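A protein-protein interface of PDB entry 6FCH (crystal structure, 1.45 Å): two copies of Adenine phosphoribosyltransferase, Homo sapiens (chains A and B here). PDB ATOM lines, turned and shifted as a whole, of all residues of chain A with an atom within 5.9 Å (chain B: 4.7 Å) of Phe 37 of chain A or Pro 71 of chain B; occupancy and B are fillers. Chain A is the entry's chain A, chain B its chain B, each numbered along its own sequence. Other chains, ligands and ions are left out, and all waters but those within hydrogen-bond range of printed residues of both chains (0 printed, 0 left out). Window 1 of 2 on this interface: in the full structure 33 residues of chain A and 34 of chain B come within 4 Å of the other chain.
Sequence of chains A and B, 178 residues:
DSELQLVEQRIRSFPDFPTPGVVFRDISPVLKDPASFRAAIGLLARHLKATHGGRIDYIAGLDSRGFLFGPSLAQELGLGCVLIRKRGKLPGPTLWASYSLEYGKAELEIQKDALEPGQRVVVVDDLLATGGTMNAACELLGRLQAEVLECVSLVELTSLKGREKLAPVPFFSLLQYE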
ATOM      1  N   VAL A  30      -4.202 -23.614 -21.757  1.00  0.00           N
ATOM      2  CA  VAL A  30      -3.214 -23.347 -22.791  1.00  0.00           C
ATOM      3  C   VAL A  30      -2.517 -24.657 -23.141  1.00  0.00           C
ATOM      4  O   VAL A  30      -2.308 -24.971 -24.303  1.00  0.00           O
ATOM      5  CB  VAL A  30      -2.162 -22.312 -22.331  1.00  0.00           C
ATOM      6  CG1 VAL A  30      -1.065 -22.169 -23.366  1.00  0.00           C
ATOM      7  CG2 VAL A  30      -2.812 -20.967 -22.073  1.00  0.00           C
ATOM      8  N   LEU A  31      -2.153 -25.418 -22.115  1.00  0.00           N
ATOM      9  CA  LEU A  31      -1.478 -26.699 -22.320  1.00  0.00           C
ATOM     10  C   LEU A  31      -2.387 -27.700 -23.029  1.00  0.00           C
ATOM     11  O   LEU A  31      -1.917 -28.528 -23.812  1.00  0.00           O
ATOM     12  CB  LEU A  31      -1.027 -27.291 -20.984  1.00  0.00           C
ATOM     13  CG  LEU A  31       0.338 -26.841 -20.443  1.00  0.00           C
ATOM     14  CD1 LEU A  31       1.470 -27.447 -21.252  1.00  0.00           C
ATOM     15  CD2 LEU A  31       0.451 -25.335 -20.405  1.00  0.00           C
ATOM     16  N   LYS A  32      -3.682 -27.639 -22.715  1.00  0.00           N
ATOM     17  CA  LYS A  32      -4.651 -28.630 -23.180  1.00  0.00           C
ATOM     18  C   LYS A  32      -5.060 -28.414 -24.633  1.00  0.00           C
ATOM     19  O   LYS A  32      -5.480 -29.350 -25.315  1.00  0.00           O
ATOM     20  CB  LYS A  32      -5.894 -28.606 -22.289  1.00  0.00           C
ATOM     21  CG  LYS A  32      -6.879 -29.723 -22.592  1.00  0.00           C
ATOM     22  CD  LYS A  32      -8.006 -29.752 -21.594  1.00  0.00           C
ATOM     23  CE  LYS A  32      -8.940 -30.901 -21.901  1.00  0.00           C
ATOM     24  NZ  LYS A  32     -10.100 -30.903 -20.975  1.00  0.00           N
ATOM     25  N   ASP A  33      -4.920 -27.175 -25.095  1.00  0.00           N
ATOM     26  CA  ASP A  33      -5.257 -26.798 -26.464  1.00  0.00           C
ATOM     27  C   ASP A  33      -3.958 -26.686 -27.265  1.00  0.00           C
ATOM     28  O   ASP A  33      -3.179 -25.761 -27.067  1.00  0.00           O
ATOM     29  CB  ASP A  33      -6.009 -25.466 -26.442  1.00  0.00           C
ATOM     30  CG  ASP A  33      -6.385 -24.974 -27.813  1.00  0.00           C
ATOM     31  OD1 ASP A  33      -5.911 -25.547 -28.813  1.00  0.00           O
ATOM     32  OD2 ASP A  33      -7.159 -23.985 -27.875  1.00  0.00           O
ATOM     33  N   PRO A  34      -3.694 -27.662 -28.144  1.00  0.00           N
ATOM     34  CA  PRO A  34      -2.380 -27.648 -28.780  1.00  0.00           C
ATOM     35  C   PRO A  34      -2.115 -26.402 -29.605  1.00  0.00           C
ATOM     36  O   PRO A  34      -0.975 -25.998 -29.741  1.00  0.00           O
ATOM     37  CB  PRO A  34      -2.377 -28.917 -29.644  1.00  0.00           C
ATOM     38  CG  PRO A  34      -3.812 -29.285 -29.812  1.00  0.00           C
ATOM     39  CD  PRO A  34      -4.542 -28.774 -28.616  1.00  0.00           C
ATOM     40  N   ALA A  35      -3.156 -25.786 -30.146  1.00  0.00           N
ATOM     41  CA  ALA A  35      -2.970 -24.578 -30.928  1.00  0.00           C
ATOM     42  C   ALA A  35      -2.547 -23.424 -30.026  1.00  0.00           C
ATOM     43  O   ALA A  35      -1.734 -22.569 -30.414  1.00  0.00           O
ATOM     44  CB  ALA A  35      -4.254 -24.235 -31.667  1.00  0.00           C
ATOM     45  N   SER A  36      -3.134 -23.383 -28.841  1.00  0.00           N
ATOM     46  CA  SER A  36      -2.841 -22.347 -27.856  1.00  0.00           C
ATOM     47  C   SER A  36      -1.409 -22.498 -27.373  1.00  0.00           C
ATOM     48  O   SER A  36      -0.666 -21.524 -27.271  1.00  0.00           O
ATOM     49  CB  SER A  36      -3.810 -22.459 -26.686  1.00  0.00           C
ATOM     50  OG  SER A  36      -3.647 -21.399 -25.759  1.00  0.00           O
ATOM     51  N   PHE A  37      -1.026 -23.731 -27.061  1.00  0.00           N
ATOM     52  CA  PHE A  37       0.324 -23.984 -26.588  1.00  0.00           C
ATOM     53  C   PHE A  37       1.335 -23.607 -27.665  1.00  0.00           C
ATOM     54  O   PHE A  37       2.329 -22.938 -27.402  1.00  0.00           O
ATOM     55  CB  PHE A  37       0.494 -25.454 -26.163  1.00  0.00           C
ATOM     56  CG  PHE A  37       1.841 -25.747 -25.560  1.00  0.00           C
ATOM     57  CD1 PHE A  37       2.125 -25.385 -24.258  1.00  0.00           C
ATOM     58  CD2 PHE A  37       2.828 -26.333 -26.313  1.00  0.00           C
ATOM     59  CE1 PHE A  37       3.374 -25.634 -23.710  1.00  0.00           C
ATOM     60  CE2 PHE A  37       4.084 -26.584 -25.774  1.00  0.00           C
ATOM     61  CZ  PHE A  37       4.351 -26.225 -24.473  1.00  0.00           C
ATOM     62  N   ARG A  38       1.078 -24.033 -28.889  1.00  0.00           N
ATOM     63  CA  ARG A  38       1.973 -23.711 -29.986  1.00  0.00           C
ATOM     64  C   ARG A  38       2.092 -22.192 -30.146  1.00  0.00           C
ATOM     65  O   ARG A  38       3.175 -21.663 -30.412  1.00  0.00           O
ATOM     66  CB  ARG A  38       1.457 -24.340 -31.278  1.00  0.00           C
ATOM     67  CG  ARG A  38       2.324 -24.063 -32.489  1.00  0.00           C
ATOM     68  CD  ARG A  38       1.845 -24.863 -33.694  1.00  0.00           C
ATOM     69  NE  ARG A  38       0.516 -24.451 -34.146  1.00  0.00           N
ATOM     70  CZ  ARG A  38      -0.604 -25.148 -33.944  1.00  0.00           C
ATOM     71  NH1 ARG A  38      -1.761 -24.686 -34.401  1.00  0.00           N
ATOM     72  NH2 ARG A  38      -0.571 -26.304 -33.292  1.00  0.00           N
ATOM     73  N   ALA A  39       0.973 -21.491 -29.999  1.00  0.00           N
ATOM     74  CA  ALA A  39       0.994 -20.043 -30.120  1.00  0.00           C
ATOM     75  C   ALA A  39       1.862 -19.417 -29.040  1.00  0.00           C
ATOM     76  O   ALA A  39       2.643 -18.503 -29.309  1.00  0.00           O
ATOM     77  CB  ALA A  39      -0.408 -19.476 -30.065  1.00  0.00           C
ATOM     78  N   ALA A  40       1.716 -19.892 -27.808  1.00  0.00           N
ATOM     79  CA  ALA A  40       2.456 -19.302 -26.705  1.00  0.00           C
ATOM     80  C   ALA A  40       3.950 -19.468 -26.948  1.00  0.00           C
ATOM     81  O   ALA A  40       4.734 -18.521 -26.801  1.00  0.00           O
ATOM     82  CB  ALA A  40       2.048 -19.955 -25.385  1.00  0.00           C
ATOM     83  N   ILE A  41       4.350 -20.684 -27.299  1.00  0.00           N
ATOM     84  CA  ILE A  41       5.754 -20.967 -27.531  1.00  0.00           C
ATOM     85  C   ILE A  41       6.256 -20.121 -28.700  1.00  0.00           C
ATOM     86  O   ILE A  41       7.335 -19.562 -28.645  1.00  0.00           O
ATOM     87  CB  ILE A  41       5.994 -22.467 -27.795  1.00  0.00           C
ATOM     88  CG1 ILE A  41       5.652 -23.303 -26.539  1.00  0.00           C
ATOM     89  CG2 ILE A  41       7.432 -22.719 -28.221  1.00  0.00           C
ATOM     90  CD1 ILE A  41       6.455 -22.952 -25.300  1.00  0.00           C
ATOM     91  N   GLY A  42       5.453 -20.019 -29.749  1.00  0.00           N
ATOM     92  CA  GLY A  42       5.847 -19.274 -30.944  1.00  0.00           C
ATOM     93  C   GLY A  42       6.019 -17.791 -30.666  1.00  0.00           C
ATOM     94  O   GLY A  42       6.963 -17.158 -31.154  1.00  0.00           O
ATOM     95  N   PHE A  67       8.696 -25.712 -16.154  1.00  0.00           N
ATOM     96  CA  PHE A  67       9.127 -26.913 -16.872  1.00  0.00           C
ATOM     97  C   PHE A  67       8.204 -27.201 -18.043  1.00  0.00           C
ATOM     98  O   PHE A  67       8.576 -27.894 -18.974  1.00  0.00           O
ATOM     99  CB  PHE A  67       9.103 -28.138 -15.952  1.00  0.00           C
ATOM    100  CG  PHE A  67      10.252 -28.232 -14.981  1.00  0.00           C
ATOM    101  CD1 PHE A  67      11.297 -27.320 -14.977  1.00  0.00           C
ATOM    102  CD2 PHE A  67      10.294 -29.292 -14.100  1.00  0.00           C
ATOM    103  CE1 PHE A  67      12.350 -27.457 -14.086  1.00  0.00           C
ATOM    104  CE2 PHE A  67      11.333 -29.439 -13.214  1.00  0.00           C
ATOM    105  CZ  PHE A  67      12.367 -28.519 -13.212  1.00  0.00           C
ATOM    106  N   LEU A  68       6.967 -26.738 -17.955  1.00  0.00           N
ATOM    107  CA  LEU A  68       6.002 -27.005 -19.016  1.00  0.00           C
ATOM    108  C   LEU A  68       6.320 -26.227 -20.276  1.00  0.00           C
ATOM    109  O   LEU A  68       5.874 -26.587 -21.365  1.00  0.00           O
ATOM    110  CB  LEU A  68       4.602 -26.640 -18.565  1.00  0.00           C
ATOM    111  CG  LEU A  68       4.018 -27.473 -17.429  1.00  0.00           C
ATOM    112  CD1 LEU A  68       2.853 -26.712 -16.813  1.00  0.00           C
ATOM    113  CD2 LEU A  68       3.582 -28.834 -17.941  1.00  0.00           C
ATOM    114  N   PHE A  69       7.062 -25.142 -20.118  1.00  0.00           N
ATOM    115  CA  PHE A  69       7.363 -24.274 -21.240  1.00  0.00           C
ATOM    116  C   PHE A  69       8.836 -24.300 -21.661  1.00  0.00           C
ATOM    117  O   PHE A  69       9.139 -24.118 -22.839  1.00  0.00           O
ATOM    118  CB  PHE A  69       6.907 -22.855 -20.932  1.00  0.00           C
ATOM    119  CG  PHE A  69       5.444 -22.767 -20.659  1.00  0.00           C
ATOM    120  CD1 PHE A  69       4.538 -22.708 -21.700  1.00  0.00           C
ATOM    121  CD2 PHE A  69       4.967 -22.838 -19.376  1.00  0.00           C
ATOM    122  CE1 PHE A  69       3.174 -22.688 -21.454  1.00  0.00           C
ATOM    123  CE2 PHE A  69       3.608 -22.814 -19.120  1.00  0.00           C
ATOM    124  CZ  PHE A  69       2.711 -22.736 -20.154  1.00  0.00           C
ATOM    125  N   SER A  72      10.015 -26.880 -24.607  1.00  0.00           N
ATOM    126  CA  SER A  72       9.389 -26.551 -25.888  1.00  0.00           C
ATOM    127  C   SER A  72       9.957 -25.257 -26.458  1.00  0.00           C
ATOM    128  O   SER A  72      10.237 -25.159 -27.649  1.00  0.00           O
ATOM    129  CB  SER A  72       7.866 -26.435 -25.736  1.00  0.00           C
ATOM    130  OG  SER A  72       7.288 -27.715 -25.498  1.00  0.00           O
ATOM    131  N   GLY B  66       7.959 -34.927 -15.148  1.00  0.00           N
ATOM    132  CA  GLY B  66       7.141 -35.318 -16.287  1.00  0.00           C
ATOM    133  C   GLY B  66       6.664 -34.124 -17.097  1.00  0.00           C
ATOM    134  O   GLY B  66       6.383 -34.238 -18.288  1.00  0.00           O
ATOM    135  N   PHE B  67       6.560 -32.976 -16.445  1.00  0.00           N
ATOM    136  CA  PHE B  67       6.203 -31.743 -17.136  1.00  0.00           C
ATOM    137  C   PHE B  67       7.208 -31.382 -18.212  1.00  0.00           C
ATOM    138  O   PHE B  67       6.900 -30.629 -19.124  1.00  0.00           O
ATOM    139  CB  PHE B  67       6.144 -30.561 -16.162  1.00  0.00           C
ATOM    140  CG  PHE B  67       4.932 -30.533 -15.276  1.00  0.00           C
ATOM    141  CD1 PHE B  67       3.920 -31.469 -15.389  1.00  0.00           C
ATOM    142  CD2 PHE B  67       4.795 -29.516 -14.348  1.00  0.00           C
ATOM    143  CE1 PHE B  67       2.800 -31.397 -14.585  1.00  0.00           C
ATOM    144  CE2 PHE B  67       3.667 -29.434 -13.549  1.00  0.00           C
ATOM    145  CZ  PHE B  67       2.672 -30.372 -13.663  1.00  0.00           C
ATOM    146  N   PHE B  69       8.486 -33.280 -20.329  1.00  0.00           N
ATOM    147  CA  PHE B  69       8.289 -34.104 -21.520  1.00  0.00           C
ATOM    148  C   PHE B  69       6.861 -34.081 -22.062  1.00  0.00           C
ATOM    149  O   PHE B  69       6.657 -34.204 -23.266  1.00  0.00           O
ATOM    150  CB  PHE B  69       8.714 -35.532 -21.222  1.00  0.00           C
ATOM    151  CG  PHE B  69      10.155 -35.638 -20.861  1.00  0.00           C
ATOM    152  CD1 PHE B  69      11.127 -35.599 -21.847  1.00  0.00           C
ATOM    153  CD2 PHE B  69      10.543 -35.651 -19.539  1.00  0.00           C
ATOM    154  CE1 PHE B  69      12.469 -35.632 -21.519  1.00  0.00           C
ATOM    155  CE2 PHE B  69      11.874 -35.699 -19.203  1.00  0.00           C
ATOM    156  CZ  PHE B  69      12.841 -35.696 -20.189  1.00  0.00           C
ATOM    157  N   GLY B  70       5.884 -33.912 -21.180  1.00  0.00           N
ATOM    158  CA  GLY B  70       4.478 -34.005 -21.586  1.00  0.00           C
ATOM    159  C   GLY B  70       4.099 -33.066 -22.713  1.00  0.00           C
ATOM    160  O   GLY B  70       3.571 -33.504 -23.735  1.00  0.00           O
ATOM    161  N   PRO B  71       4.347 -31.766 -22.541  1.00  0.00           N
ATOM    162  CA  PRO B  71       3.916 -30.835 -23.581  1.00  0.00           C
ATOM    163  C   PRO B  71       4.592 -31.079 -24.928  1.00  0.00           C
ATOM    164  O   PRO B  71       3.929 -31.075 -25.956  1.00  0.00           O
ATOM    165  CB  PRO B  71       4.287 -29.468 -22.999  1.00  0.00           C
ATOM    166  CG  PRO B  71       4.196 -29.677 -21.520  1.00  0.00           C
ATOM    167  CD  PRO B  71       4.724 -31.062 -21.296  1.00  0.00           C
ATOM    168  N   SER B  72       5.893 -31.340 -24.924  1.00  0.00           N
ATOM    169  CA  SER B  72       6.595 -31.594 -26.173  1.00  0.00           C
ATOM    170  C   SER B  72       6.079 -32.848 -26.863  1.00  0.00           C
ATOM    171  O   SER B  72       5.936 -32.881 -28.087  1.00  0.00           O
ATOM    172  CB  SER B  72       8.091 -31.723 -25.926  1.00  0.00           C
ATOM    173  OG  SER B  72       8.643 -30.474 -25.555  1.00  0.00           O
ATOM    174  N   LEU B  73       5.817 -33.888 -26.079  1.00  0.00           N
ATOM    175  CA  LEU B  73       5.298 -35.132 -26.627  1.00  0.00           C
ATOM    176  C   LEU B  73       3.910 -34.909 -27.210  1.00  0.00           C
ATOM    177  O   LEU B  73       3.609 -35.332 -28.340  1.00  0.00           O
ATOM    178  CB  LEU B  73       5.265 -36.220 -25.550  1.00  0.00           C
ATOM    179  CG  LEU B  73       4.734 -37.587 -25.988  1.00  0.00           C
ATOM    180  CD1 LEU B  73       5.492 -38.103 -27.217  1.00  0.00           C
ATOM    181  CD2 LEU B  73       4.832 -38.566 -24.829  1.00  0.00           C
ATOM    182  N   ALA B  74       3.060 -34.241 -26.452  1.00  0.00           N
ATOM    183  CA  ALA B  74       1.726 -33.888 -26.931  1.00  0.00           C
ATOM    184  C   ALA B  74       1.823 -33.104 -28.241  1.00  0.00           C
ATOM    185  O   ALA B  74       1.143 -33.422 -29.231  1.00  0.00           O
ATOM    186  CB  ALA B  74       0.983 -33.077 -25.865  1.00  0.00           C
ATOM    187  N   GLN B  75       2.641 -32.069 -28.243  1.00  0.00           N
ATOM    188  CA  GLN B  75       2.820 -31.257 -29.443  1.00  0.00           C
ATOM    189  C   GLN B  75       3.225 -32.116 -30.644  1.00  0.00           C
ATOM    190  O   GLN B  75       2.682 -31.955 -31.748  1.00  0.00           O
ATOM    191  CB  GLN B  75       3.847 -30.165 -29.199  1.00  0.00           C
ATOM    192  CG  GLN B  75       3.276 -28.937 -28.512  1.00  0.00           C
ATOM    193  CD  GLN B  75       2.421 -28.089 -29.449  1.00  0.00           C
ATOM    194  OE1 GLN B  75       2.920 -27.528 -30.421  1.00  0.00           O
ATOM    195  NE2 GLN B  75       1.133 -28.015 -29.174  1.00  0.00           N
ATOM    196  N   CYS B  81      -2.028 -31.431 -23.735  1.00  0.00           N
ATOM    197  CA  CYS B  81      -1.485 -32.052 -22.549  1.00  0.00           C
ATOM    198  C   CYS B  81      -2.282 -31.609 -21.336  1.00  0.00           C
ATOM    199  O   CYS B  81      -2.486 -30.415 -21.116  1.00  0.00           O
ATOM    200  CB  CYS B  81      -0.029 -31.642 -22.383  1.00  0.00           C
ATOM    201  SG  CYS B  81       0.860 -32.523 -21.082  1.00  0.00           S
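Phe 67 of chain B touches its own counterpart, Phe 67 of chain A. Ser 72 of chain A touches its own counterpart, Ser 72 of chain B. Positions printed for both chains: 67, 69 and 72. Of the 11 pairs that touch across the chains among the printed residues, 2 have their exchanged pair printed and touching as well.
Hydrophobic or aromatic side chains of chain B within 4 Å of the printed part of chain A: Phe 67 and Pro 71. Hydrophobic or aromatic side chains of chain A that line the printed part of chain B: Leu 31, Pro 34, Phe 37, Phe 67 and Leu 68.
Phe 37 of chain A touches just these residues of chain B: Pro 71 (3.6 Å) and Gln 75 (3.4 Å). Of chain A, only Leu 31 (3.5 Å), Phe 37 (3.6 Å) and Leu 68 (3.5 Å) come within 4 Å of Pro 71 of chain B. Printed residues of chain B within 4 Å of Arg 38 of chain A: Gln 75. Printed residues of chain B within 4 Å of Leu 31 of chain A: Pro 71 and Cys 81. Of the printed residues of chain B, Lys 32 of chain A touches Cys 81 (3.4 Å). Of the printed residues of chain B, Leu 68 of chain A touches Phe 67 and Pro 71. Printed residues of chain A within 4 Å of Ser 72 of chain B: Ser 72 (3.1 Å). Asp 33 of chain A touches none of the printed residues of chain B. Phe 69 of chain B touches none of the printed residues of chain A. The nearest printed residue of chain A that does not touch Ser 72 of chain B is Phe 37 of chain A (5.2 Å).
The backbone NH of Phe 37 of chain A lies within hydrogen-bond range of the backbone carbonyl oxygen of Val 30 of chain A, 3.3 Å away.
CG of Pro 71 of chain B touches CD1 of Leu 31 of chain A (3.5 Å). CB of Pro 71 of chain B touches CZ of Phe 37 of chain A, at 3.6 Å. Gln 75 of chain B touches Phe 37 of chain A. Arg 38 of chain A touches Gln 75 of chain B. Leu 68 of chain A touches Phe 67 of chain B. CG of Pro 71 of chain B touches O of Leu 68 of chain A, 3.5 Å away.
The backbone carbonyl oxygen (O) of Pro 34 of chain A lies within hydrogen-bond range of the side-chain amide nitrogen (NE2) of Gln 75 of chain B, at 3.0 Å. The backbone carbonyl oxygen of Phe 67 of chain B sits close to the backbone carbonyl oxygen of Phe 67 of chain A. The side-chain hydroxyl (OG) of Ser 72 of chain A sits at hydrogen-bond distance from the side-chain hydroxyl (OG) of Ser 72 of chain B. The backbone NH (N) of Lys 32 of chain A lies within hydrogen-bond range of the backbone carbonyl oxygen (O) of Cys 81 of chain B (3.4 Å). The backbone carbonyl oxygen (O) of Leu 31 of chain A sits at hydrogen-bond distance from the backbone NH (N) of Cys 81 of chain B.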
